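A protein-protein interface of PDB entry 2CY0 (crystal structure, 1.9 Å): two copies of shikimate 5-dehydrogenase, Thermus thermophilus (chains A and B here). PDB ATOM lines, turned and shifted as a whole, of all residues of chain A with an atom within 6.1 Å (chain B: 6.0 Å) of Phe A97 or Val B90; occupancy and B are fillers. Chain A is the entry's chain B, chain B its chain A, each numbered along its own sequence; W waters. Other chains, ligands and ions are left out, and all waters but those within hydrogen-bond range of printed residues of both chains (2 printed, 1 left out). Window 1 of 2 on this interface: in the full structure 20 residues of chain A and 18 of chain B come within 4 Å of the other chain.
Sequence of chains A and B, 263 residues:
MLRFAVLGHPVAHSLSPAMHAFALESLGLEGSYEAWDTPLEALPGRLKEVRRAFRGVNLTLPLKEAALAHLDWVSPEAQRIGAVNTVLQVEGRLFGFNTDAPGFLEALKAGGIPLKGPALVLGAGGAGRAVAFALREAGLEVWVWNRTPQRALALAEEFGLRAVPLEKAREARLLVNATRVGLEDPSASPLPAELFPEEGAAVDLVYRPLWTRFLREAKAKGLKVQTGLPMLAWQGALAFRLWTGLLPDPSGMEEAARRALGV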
ATOM      1  N   LEU A  71     -27.482  20.712   0.069  1.00  0.00           N
ATOM      2  CA  LEU A  71     -28.153  21.478  -0.980  1.00  0.00           C
ATOM      3  C   LEU A  71     -29.667  21.563  -0.826  1.00  0.00           C
ATOM      4  O   LEU A  71     -30.300  20.679  -0.249  1.00  0.00           O
ATOM      5  CB  LEU A  71     -27.806  20.892  -2.354  1.00  0.00           C
ATOM      6  CG  LEU A  71     -26.313  20.610  -2.577  1.00  0.00           C
ATOM      7  CD1 LEU A  71     -26.086  20.076  -3.991  1.00  0.00           C
ATOM      8  CD2 LEU A  71     -25.506  21.882  -2.330  1.00  0.00           C
ATOM      9  N   TRP A  73     -31.721  21.503  -3.292  1.00  0.00           N
ATOM     10  CA  TRP A  73     -32.319  20.641  -4.302  1.00  0.00           C
ATOM     11  C   TRP A  73     -31.222  19.896  -5.048  1.00  0.00           C
ATOM     12  O   TRP A  73     -30.218  20.492  -5.441  1.00  0.00           O
ATOM     13  CB  TRP A  73     -33.112  21.480  -5.300  1.00  0.00           C
ATOM     14  CG  TRP A  73     -33.868  20.679  -6.329  1.00  0.00           C
ATOM     15  CD1 TRP A  73     -35.149  20.220  -6.229  1.00  0.00           C
ATOM     16  CD2 TRP A  73     -33.397  20.272  -7.623  1.00  0.00           C
ATOM     17  NE1 TRP A  73     -35.511  19.559  -7.381  1.00  0.00           N
ATOM     18  CE2 TRP A  73     -34.453  19.575  -8.252  1.00  0.00           C
ATOM     19  CE3 TRP A  73     -32.185  20.430  -8.314  1.00  0.00           C
ATOM     20  CZ2 TRP A  73     -34.337  19.035  -9.540  1.00  0.00           C
ATOM     21  CZ3 TRP A  73     -32.070  19.892  -9.599  1.00  0.00           C
ATOM     22  CH2 TRP A  73     -33.142  19.205 -10.195  1.00  0.00           C
ATOM     23  N   VAL A  74     -31.416  18.595  -5.240  1.00  0.00           N
ATOM     24  CA  VAL A  74     -30.447  17.777  -5.956  1.00  0.00           C
ATOM     25  C   VAL A  74     -31.147  17.099  -7.110  1.00  0.00           C
ATOM     26  O   VAL A  74     -32.206  16.498  -6.935  1.00  0.00           O
ATOM     27  CB  VAL A  74     -29.837  16.680  -5.060  1.00  0.00           C
ATOM     28  CG1 VAL A  74     -28.850  15.849  -5.865  1.00  0.00           C
ATOM     29  CG2 VAL A  74     -29.145  17.307  -3.859  1.00  0.00           C
ATOM     30  N   SER A  75     -30.553  17.191  -8.294  1.00  0.00           N
ATOM     31  CA  SER A  75     -31.142  16.569  -9.467  1.00  0.00           C
ATOM     32  C   SER A  75     -31.264  15.073  -9.212  1.00  0.00           C
ATOM     33  O   SER A  75     -30.560  14.513  -8.370  1.00  0.00           O
ATOM     34  CB  SER A  75     -30.272  16.806 -10.707  1.00  0.00           C
ATOM     35  OG  SER A  75     -29.176  15.906 -10.744  1.00  0.00           O
ATOM     36  N   ALA A  78     -28.156  13.148 -10.247  1.00  0.00           N
ATOM     37  CA  ALA A  78     -27.159  13.365  -9.211  1.00  0.00           C
ATOM     38  C   ALA A  78     -27.558  12.603  -7.942  1.00  0.00           C
ATOM     39  O   ALA A  78     -26.702  12.219  -7.146  1.00  0.00           O
ATOM     40  CB  ALA A  78     -27.023  14.863  -8.919  1.00  0.00           C
ATOM     41  N   ALA A  83     -23.590  11.689  -6.462  1.00  0.00           N
ATOM     42  CA  ALA A  83     -22.524  12.676  -6.520  1.00  0.00           C
ATOM     43  C   ALA A  83     -22.955  13.928  -7.275  1.00  0.00           C
ATOM     44  O   ALA A  83     -23.734  13.860  -8.220  1.00  0.00           O
ATOM     45  CB  ALA A  83     -21.294  12.068  -7.181  1.00  0.00           C
ATOM     46  N   VAL A  84     -22.447  15.071  -6.833  1.00  0.00           N
ATOM     47  CA  VAL A  84     -22.738  16.350  -7.465  1.00  0.00           C
ATOM     48  C   VAL A  84     -21.410  17.019  -7.831  1.00  0.00           C
ATOM     49  O   VAL A  84     -20.527  17.173  -6.979  1.00  0.00           O
ATOM     50  CB  VAL A  84     -23.529  17.282  -6.516  1.00  0.00           C
ATOM     51  CG1 VAL A  84     -23.544  18.696  -7.062  1.00  0.00           C
ATOM     52  CG2 VAL A  84     -24.960  16.777  -6.369  1.00  0.00           C
ATOM     53  N   ASN A  85     -21.271  17.403  -9.097  1.00  0.00           N
ATOM     54  CA  ASN A  85     -20.055  18.058  -9.578  1.00  0.00           C
ATOM     55  C   ASN A  85     -20.338  19.513  -9.934  1.00  0.00           C
ATOM     56  O   ASN A  85     -19.418  20.310 -10.122  1.00  0.00           O
ATOM     57  CB  ASN A  85     -19.524  17.340 -10.820  1.00  0.00           C
ATOM     58  CG  ASN A  85     -20.265  17.739 -12.089  1.00  0.00           C
ATOM     59  OD1 ASN A  85     -21.489  17.864 -12.097  1.00  0.00           O
ATOM     60  ND2 ASN A  85     -19.518  17.936 -13.171  1.00  0.00           N
ATOM     61  N   THR A  86     -21.619  19.858 -10.020  1.00  0.00           N
ATOM     62  CA  THR A  86     -22.006  21.213 -10.379  1.00  0.00           C
ATOM     63  C   THR A  86     -23.098  21.791  -9.490  1.00  0.00           C
ATOM     64  O   THR A  86     -24.189  21.236  -9.376  1.00  0.00           O
ATOM     65  CB  THR A  86     -22.462  21.266 -11.845  1.00  0.00           C
ATOM     66  OG1 THR A  86     -21.432  20.713 -12.678  1.00  0.00           O
ATOM     67  CG2 THR A  86     -22.739  22.702 -12.266  1.00  0.00           C
ATOM     68  N   VAL A  87     -22.784  22.921  -8.865  1.00  0.00           N
ATOM     69  CA  VAL A  87     -23.717  23.605  -7.983  1.00  0.00           C
ATOM     70  C   VAL A  87     -24.058  24.980  -8.550  1.00  0.00           C
ATOM     71  O   VAL A  87     -23.170  25.725  -8.963  1.00  0.00           O
ATOM     72  CB  VAL A  87     -23.115  23.785  -6.568  1.00  0.00           C
ATOM     73  CG1 VAL A  87     -24.096  24.526  -5.670  1.00  0.00           C
ATOM     74  CG2 VAL A  87     -22.774  22.425  -5.973  1.00  0.00           C
ATOM     75  N   LEU A  88     -25.352  25.293  -8.568  1.00  0.00           N
ATOM     76  CA  LEU A  88     -25.875  26.567  -9.061  1.00  0.00           C
ATOM     77  C   LEU A  88     -26.476  27.354  -7.899  1.00  0.00           C
ATOM     78  O   LEU A  88     -27.224  26.795  -7.096  1.00  0.00           O
ATOM     79  CB  LEU A  88     -26.970  26.316 -10.107  1.00  0.00           C
ATOM     80  CG  LEU A  88     -27.886  27.498 -10.439  1.00  0.00           C
ATOM     81  CD1 LEU A  88     -27.085  28.617 -11.090  1.00  0.00           C
ATOM     82  CD2 LEU A  88     -28.993  27.031 -11.374  1.00  0.00           C
ATOM     83  N   PHE A  95     -28.492  24.552  -5.826  1.00  0.00           N
ATOM     84  CA  PHE A  95     -29.023  23.420  -6.582  1.00  0.00           C
ATOM     85  C   PHE A  95     -27.850  22.566  -7.079  1.00  0.00           C
ATOM     86  O   PHE A  95     -26.856  23.102  -7.578  1.00  0.00           O
ATOM     87  CB  PHE A  95     -29.826  23.924  -7.776  1.00  0.00           C
ATOM     88  CG  PHE A  95     -31.014  24.759  -7.400  1.00  0.00           C
ATOM     89  CD1 PHE A  95     -32.151  24.174  -6.870  1.00  0.00           C
ATOM     90  CD2 PHE A  95     -30.989  26.135  -7.563  1.00  0.00           C
ATOM     91  CE1 PHE A  95     -33.259  24.945  -6.523  1.00  0.00           C
ATOM     92  CE2 PHE A  95     -32.090  26.916  -7.219  1.00  0.00           C
ATOM     93  CZ  PHE A  95     -33.225  26.319  -6.693  1.00  0.00           C
ATOM     94  N   GLY A  96     -27.971  21.246  -6.947  1.00  0.00           N
ATOM     95  CA  GLY A  96     -26.900  20.362  -7.379  1.00  0.00           C
ATOM     96  C   GLY A  96     -27.213  19.517  -8.601  1.00  0.00           C
ATOM     97  O   GLY A  96     -28.319  18.991  -8.740  1.00  0.00           O
ATOM     98  N   PHE A  97     -26.232  19.394  -9.495  1.00  0.00           N
ATOM     99  CA  PHE A  97     -26.380  18.597 -10.710  1.00  0.00           C
ATOM    100  C   PHE A  97     -25.113  17.790 -10.982  1.00  0.00           C
ATOM    101  O   PHE A  97     -24.080  17.982 -10.335  1.00  0.00           O
ATOM    102  CB  PHE A  97     -26.621  19.484 -11.931  1.00  0.00           C
ATOM    103  CG  PHE A  97     -27.716  20.487 -11.762  1.00  0.00           C
ATOM    104  CD1 PHE A  97     -27.532  21.609 -10.961  1.00  0.00           C
ATOM    105  CD2 PHE A  97     -28.925  20.320 -12.416  1.00  0.00           C
ATOM    106  CE1 PHE A  97     -28.535  22.555 -10.831  1.00  0.00           C
ATOM    107  CE2 PHE A  97     -29.934  21.262 -12.288  1.00  0.00           C
ATOM    108  CZ  PHE A  97     -29.737  22.379 -11.490  1.00  0.00           C
ATOM    109  N   ASN A  98     -25.198  16.889 -11.954  1.00  0.00           N
ATOM    110  CA  ASN A  98     -24.041  16.092 -12.342  1.00  0.00           C
ATOM    111  C   ASN A  98     -23.862  16.226 -13.847  1.00  0.00           C
ATOM    112  O   ASN A  98     -24.599  15.620 -14.616  1.00  0.00           O
ATOM    113  CB  ASN A  98     -24.230  14.623 -11.976  1.00  0.00           C
ATOM    114  CG  ASN A  98     -22.956  13.823 -12.157  1.00  0.00           C
ATOM    115  OD1 ASN A  98     -22.383  13.797 -13.244  1.00  0.00           O
ATOM    116  ND2 ASN A  98     -22.499  13.180 -11.090  1.00  0.00           N
ATOM    117  N   THR A  99     -22.891  17.032 -14.270  1.00  0.00           N
ATOM    118  CA  THR A  99     -22.653  17.231 -15.698  1.00  0.00           C
ATOM    119  C   THR A  99     -21.707  16.189 -16.305  1.00  0.00           C
ATOM    120  O   THR A  99     -21.474  16.182 -17.516  1.00  0.00           O
ATOM    121  CB  THR A  99     -22.086  18.643 -15.981  1.00  0.00           C
ATOM    122  OG1 THR A  99     -20.876  18.833 -15.242  1.00  0.00           O
ATOM    123  CG2 THR A  99     -23.090  19.706 -15.586  1.00  0.00           C
ATOM    124  N   ARG A 241     -23.102  26.359 -19.184  1.00  0.00           N
ATOM    125  CA  ARG A 241     -24.434  26.601 -19.751  1.00  0.00           C
ATOM    126  C   ARG A 241     -25.445  26.624 -18.614  1.00  0.00           C
ATOM    127  O   ARG A 241     -26.373  27.440 -18.581  1.00  0.00           O
ATOM    128  CB  ARG A 241     -24.841  25.478 -20.721  1.00  0.00           C
ATOM    129  CG  ARG A 241     -26.197  25.739 -21.394  1.00  0.00           C
ATOM    130  CD  ARG A 241     -26.897  24.484 -21.912  1.00  0.00           C
ATOM    131  NE  ARG A 241     -27.958  24.853 -22.849  1.00  0.00           N
ATOM    132  CZ  ARG A 241     -29.180  24.323 -22.880  1.00  0.00           C
ATOM    133  NH1 ARG A 241     -29.536  23.379 -22.021  1.00  0.00           N
ATOM    134  NH2 ARG A 241     -30.060  24.756 -23.774  1.00  0.00           N
ATOM    135  N   LEU A 242     -25.254  25.702 -17.684  1.00  0.00           N
ATOM    136  CA  LEU A 242     -26.122  25.570 -16.535  1.00  0.00           C
ATOM    137  C   LEU A 242     -26.136  26.859 -15.697  1.00  0.00           C
ATOM    138  O   LEU A 242     -27.189  27.322 -15.261  1.00  0.00           O
ATOM    139  CB  LEU A 242     -25.633  24.386 -15.712  1.00  0.00           C
ATOM    140  CG  LEU A 242     -26.565  23.794 -14.671  1.00  0.00           C
ATOM    141  CD1 LEU A 242     -26.177  22.345 -14.419  1.00  0.00           C
ATOM    142  CD2 LEU A 242     -26.491  24.624 -13.400  1.00  0.00           C
ATOM    143  N   ARG B  55     -34.517  29.006 -21.887  1.00  0.00           N
ATOM    144  CA  ARG B  55     -33.703  29.115 -20.693  1.00  0.00           C
ATOM    145  C   ARG B  55     -34.590  29.525 -19.521  1.00  0.00           C
ATOM    146  O   ARG B  55     -34.345  29.146 -18.382  1.00  0.00           O
ATOM    147  CB  ARG B  55     -32.613  30.164 -20.922  1.00  0.00           C
ATOM    148  CG  ARG B  55     -31.824  30.552 -19.690  1.00  0.00           C
ATOM    149  CD  ARG B  55     -31.072  29.377 -19.092  1.00  0.00           C
ATOM    150  NE  ARG B  55     -30.215  29.821 -17.997  1.00  0.00           N
ATOM    151  CZ  ARG B  55     -29.447  29.017 -17.272  1.00  0.00           C
ATOM    152  NH1 ARG B  55     -29.420  27.716 -17.519  1.00  0.00           N
ATOM    153  NH2 ARG B  55     -28.708  29.516 -16.294  1.00  0.00           N
ATOM    154  N   LEU B  88     -37.046  29.198 -14.310  1.00  0.00           N
ATOM    155  CA  LEU B  88     -35.712  28.939 -14.850  1.00  0.00           C
ATOM    156  C   LEU B  88     -35.699  27.485 -15.299  1.00  0.00           C
ATOM    157  O   LEU B  88     -36.230  26.622 -14.602  1.00  0.00           O
ATOM    158  CB  LEU B  88     -34.633  29.139 -13.778  1.00  0.00           C
ATOM    159  CG  LEU B  88     -33.234  28.566 -14.060  1.00  0.00           C
ATOM    160  CD1 LEU B  88     -32.589  29.321 -15.204  1.00  0.00           C
ATOM    161  CD2 LEU B  88     -32.360  28.675 -12.815  1.00  0.00           C
ATOM    162  N   GLN B  89     -35.103  27.219 -16.458  1.00  0.00           N
ATOM    163  CA  GLN B  89     -35.017  25.852 -16.981  1.00  0.00           C
ATOM    164  C   GLN B  89     -33.565  25.415 -17.109  1.00  0.00           C
ATOM    165  O   GLN B  89     -32.769  26.070 -17.776  1.00  0.00           O
ATOM    166  CB  GLN B  89     -35.700  25.754 -18.351  1.00  0.00           C
ATOM    167  CG  GLN B  89     -35.618  24.364 -19.024  1.00  0.00           C
ATOM    168  CD  GLN B  89     -34.246  24.063 -19.607  1.00  0.00           C
ATOM    169  OE1 GLN B  89     -33.464  23.294 -19.039  1.00  0.00           O
ATOM    170  NE2 GLN B  89     -33.943  24.679 -20.744  1.00  0.00           N
ATOM    171  N   VAL B  90     -33.222  24.315 -16.450  1.00  0.00           N
ATOM    172  CA  VAL B  90     -31.871  23.771 -16.504  1.00  0.00           C
ATOM    173  C   VAL B  90     -32.000  22.256 -16.559  1.00  0.00           C
ATOM    174  O   VAL B  90     -32.720  21.663 -15.756  1.00  0.00           O
ATOM    175  CB  VAL B  90     -31.034  24.176 -15.260  1.00  0.00           C
ATOM    176  CG1 VAL B  90     -30.860  25.689 -15.214  1.00  0.00           C
ATOM    177  CG2 VAL B  90     -31.708  23.691 -13.993  1.00  0.00           C
ATOM    178  N   GLU B  91     -31.318  21.638 -17.517  1.00  0.00           N
ATOM    179  CA  GLU B  91     -31.368  20.186 -17.689  1.00  0.00           C
ATOM    180  C   GLU B  91     -32.798  19.677 -17.777  1.00  0.00           C
ATOM    181  O   GLU B  91     -33.096  18.566 -17.345  1.00  0.00           O
ATOM    182  CB  GLU B  91     -30.642  19.465 -16.544  1.00  0.00           C
ATOM    183  CG  GLU B  91     -29.126  19.457 -16.681  1.00  0.00           C
ATOM    184  CD  GLU B  91     -28.445  18.543 -15.678  1.00  0.00           C
ATOM    185  OE1 GLU B  91     -27.220  18.321 -15.814  1.00  0.00           O
ATOM    186  OE2 GLU B  91     -29.126  18.053 -14.752  1.00  0.00           O
ATOM    187  N   GLY B  92     -33.678  20.499 -18.337  1.00  0.00           N
ATOM    188  CA  GLY B  92     -35.067  20.106 -18.483  1.00  0.00           C
ATOM    189  C   GLY B  92     -35.890  20.169 -17.211  1.00  0.00           C
ATOM    190  O   GLY B  92     -37.065  19.801 -17.223  1.00  0.00           O
ATOM    191  N   ARG B  93     -35.279  20.614 -16.115  1.00  0.00           N
ATOM    192  CA  ARG B  93     -35.983  20.736 -14.842  1.00  0.00           C
ATOM    193  C   ARG B  93     -36.476  22.185 -14.727  1.00  0.00           C
ATOM    194  O   ARG B  93     -35.826  23.106 -15.225  1.00  0.00           O
ATOM    195  CB  ARG B  93     -35.045  20.400 -13.677  1.00  0.00           C
ATOM    196  CG  ARG B  93     -34.268  19.087 -13.835  1.00  0.00           C
ATOM    197  CD  ARG B  93     -35.184  17.873 -13.912  1.00  0.00           C
ATOM    198  NE  ARG B  93     -34.429  16.648 -14.161  1.00  0.00           N
ATOM    199  CZ  ARG B  93     -34.975  15.441 -14.297  1.00  0.00           C
ATOM    200  NH1 ARG B  93     -36.288  15.286 -14.208  1.00  0.00           N
ATOM    201  NH2 ARG B  93     -34.204  14.386 -14.528  1.00  0.00           N
ATOM    202  N   LEU B  94     -37.627  22.383 -14.087  1.00  0.00           N
ATOM    203  CA  LEU B  94     -38.195  23.726 -13.940  1.00  0.00           C
ATOM    204  C   LEU B  94     -38.242  24.210 -12.496  1.00  0.00           C
ATOM    205  O   LEU B  94     -38.775  23.529 -11.618  1.00  0.00           O
ATOM    206  CB  LEU B  94     -39.604  23.772 -14.536  1.00  0.00           C
ATOM    207  CG  LEU B  94     -39.698  23.510 -16.041  1.00  0.00           C
ATOM    208  CD1 LEU B  94     -41.152  23.665 -16.495  1.00  0.00           C
ATOM    209  CD2 LEU B  94     -38.783  24.483 -16.798  1.00  0.00           C
ATOM    210  N   PHE B  95     -37.686  25.397 -12.263  1.00  0.00           N
ATOM    211  CA  PHE B  95     -37.652  25.990 -10.932  1.00  0.00           C
ATOM    212  C   PHE B  95     -38.434  27.300 -10.922  1.00  0.00           C
ATOM    213  O   PHE B  95     -38.189  28.185 -11.749  1.00  0.00           O
ATOM    214  CB  PHE B  95     -36.198  26.239 -10.521  1.00  0.00           C
ATOM    215  CG  PHE B  95     -35.357  24.996 -10.514  1.00  0.00           C
ATOM    216  CD1 PHE B  95     -35.044  24.354  -9.323  1.00  0.00           C
ATOM    217  CD2 PHE B  95     -34.918  24.438 -11.708  1.00  0.00           C
ATOM    218  CE1 PHE B  95     -34.303  23.170  -9.322  1.00  0.00           C
ATOM    219  CE2 PHE B  95     -34.178  23.257 -11.717  1.00  0.00           C
ATOM    220  CZ  PHE B  95     -33.874  22.622 -10.521  1.00  0.00           C
HETATM  221  O   HOH W   1     -28.797  23.526 -18.650  1.00  0.00           O
HETATM  222  O   HOH W   2     -27.752  16.289 -13.191  1.00  0.00           O
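The guanidinium group (NH2) of Arg B55 is in hydrogen-bond range of the backbone carbonyl oxygen (O) of Leu A242 (2.9 Å). NH1 of Arg B55 is in hydrogen-bond range of O of Arg A241, 3.2 Å away.
O of Arg B55 sits at hydrogen-bond distance from N of Gln B89, 2.8 Å away. The backbone NH of Leu A88 lies within hydrogen-bond range of the backbone carbonyl oxygen of Phe A95 (2.8 Å). O of Phe A97 sits at hydrogen-bond distance from N of Asn A85. The backbone NH (N) of Glu B91 sits at hydrogen-bond distance from the side-chain amide oxygen (OE1) of Gln B89 (3.1 Å). O of Thr A86 sits at hydrogen-bond distance from N of Phe A97 (2.8 Å). The backbone carbonyl oxygen of Ala A83 lies within hydrogen-bond range of the side-chain amide nitrogen of Asn A98 (3.2 Å).
Trp A73 touches Arg B93 (CH2 to CG, 3.8 Å). CZ3 of Trp A73 touches CZ of Phe B95 (3.4 Å). Phe B95 touches Phe A95. CG2 of Val B90 touches CZ of Phe A97 (3.4 Å). Phe A97 touches Glu B91 (CD2 to OE2, 3.3 Å). Glu B91 touches Asn A98.
Phe A97 touches just these residues of chain B: Val B90 (3.4 Å) and Glu B91 (3.3 Å). Of the printed residues of chain B, Asn A98 touches Glu B91 (3.9 Å). Of the printed residues of chain A, Val B90 touches Phe A97. Printed residues of chain A within 4 Å of Arg B93: Trp A73 (3.8 Å). The nearest residue of chain B that does not touch Phe A97 is Phe B95 (4.3 Å). The nearest printed residue of chain A that does not touch Val B90 is Leu A242 (4.02 Å). The nearest printed residue of chain A that does not touch Arg B55 is Leu A88 (5.5 Å).
Hydrophobic or aromatic side chains of chain A within 4 Å of the printed part of chain B: Trp A73, Phe A95 and Phe A97. Printed residues of chain B that touch a printed residue of chain A: Arg B55, Val B90, Glu B91, Arg B93 and Phe B95. Along chain B the printed residues that touch a printed residue of chain A span positions 55 to 95. Among the printed residues, no Asp or Glu carboxylate lies within 4 Å of a Lys or Arg side-chain nitrogen of the other chain.
Phe A95 touches its own counterpart, Phe B95.
Water W2 lies within hydrogen-bond range of OE2 of Glu B91 (2.7 Å), OG of Ser A75 (2.9 Å) and N of Asn A98 (2.9 Å). Water W1 lies within hydrogen-bond range of the backbone NH (N) of Glu B91 (3.3 Å) and the guanidinium group (NH1) of Arg A241 (3.5 Å).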
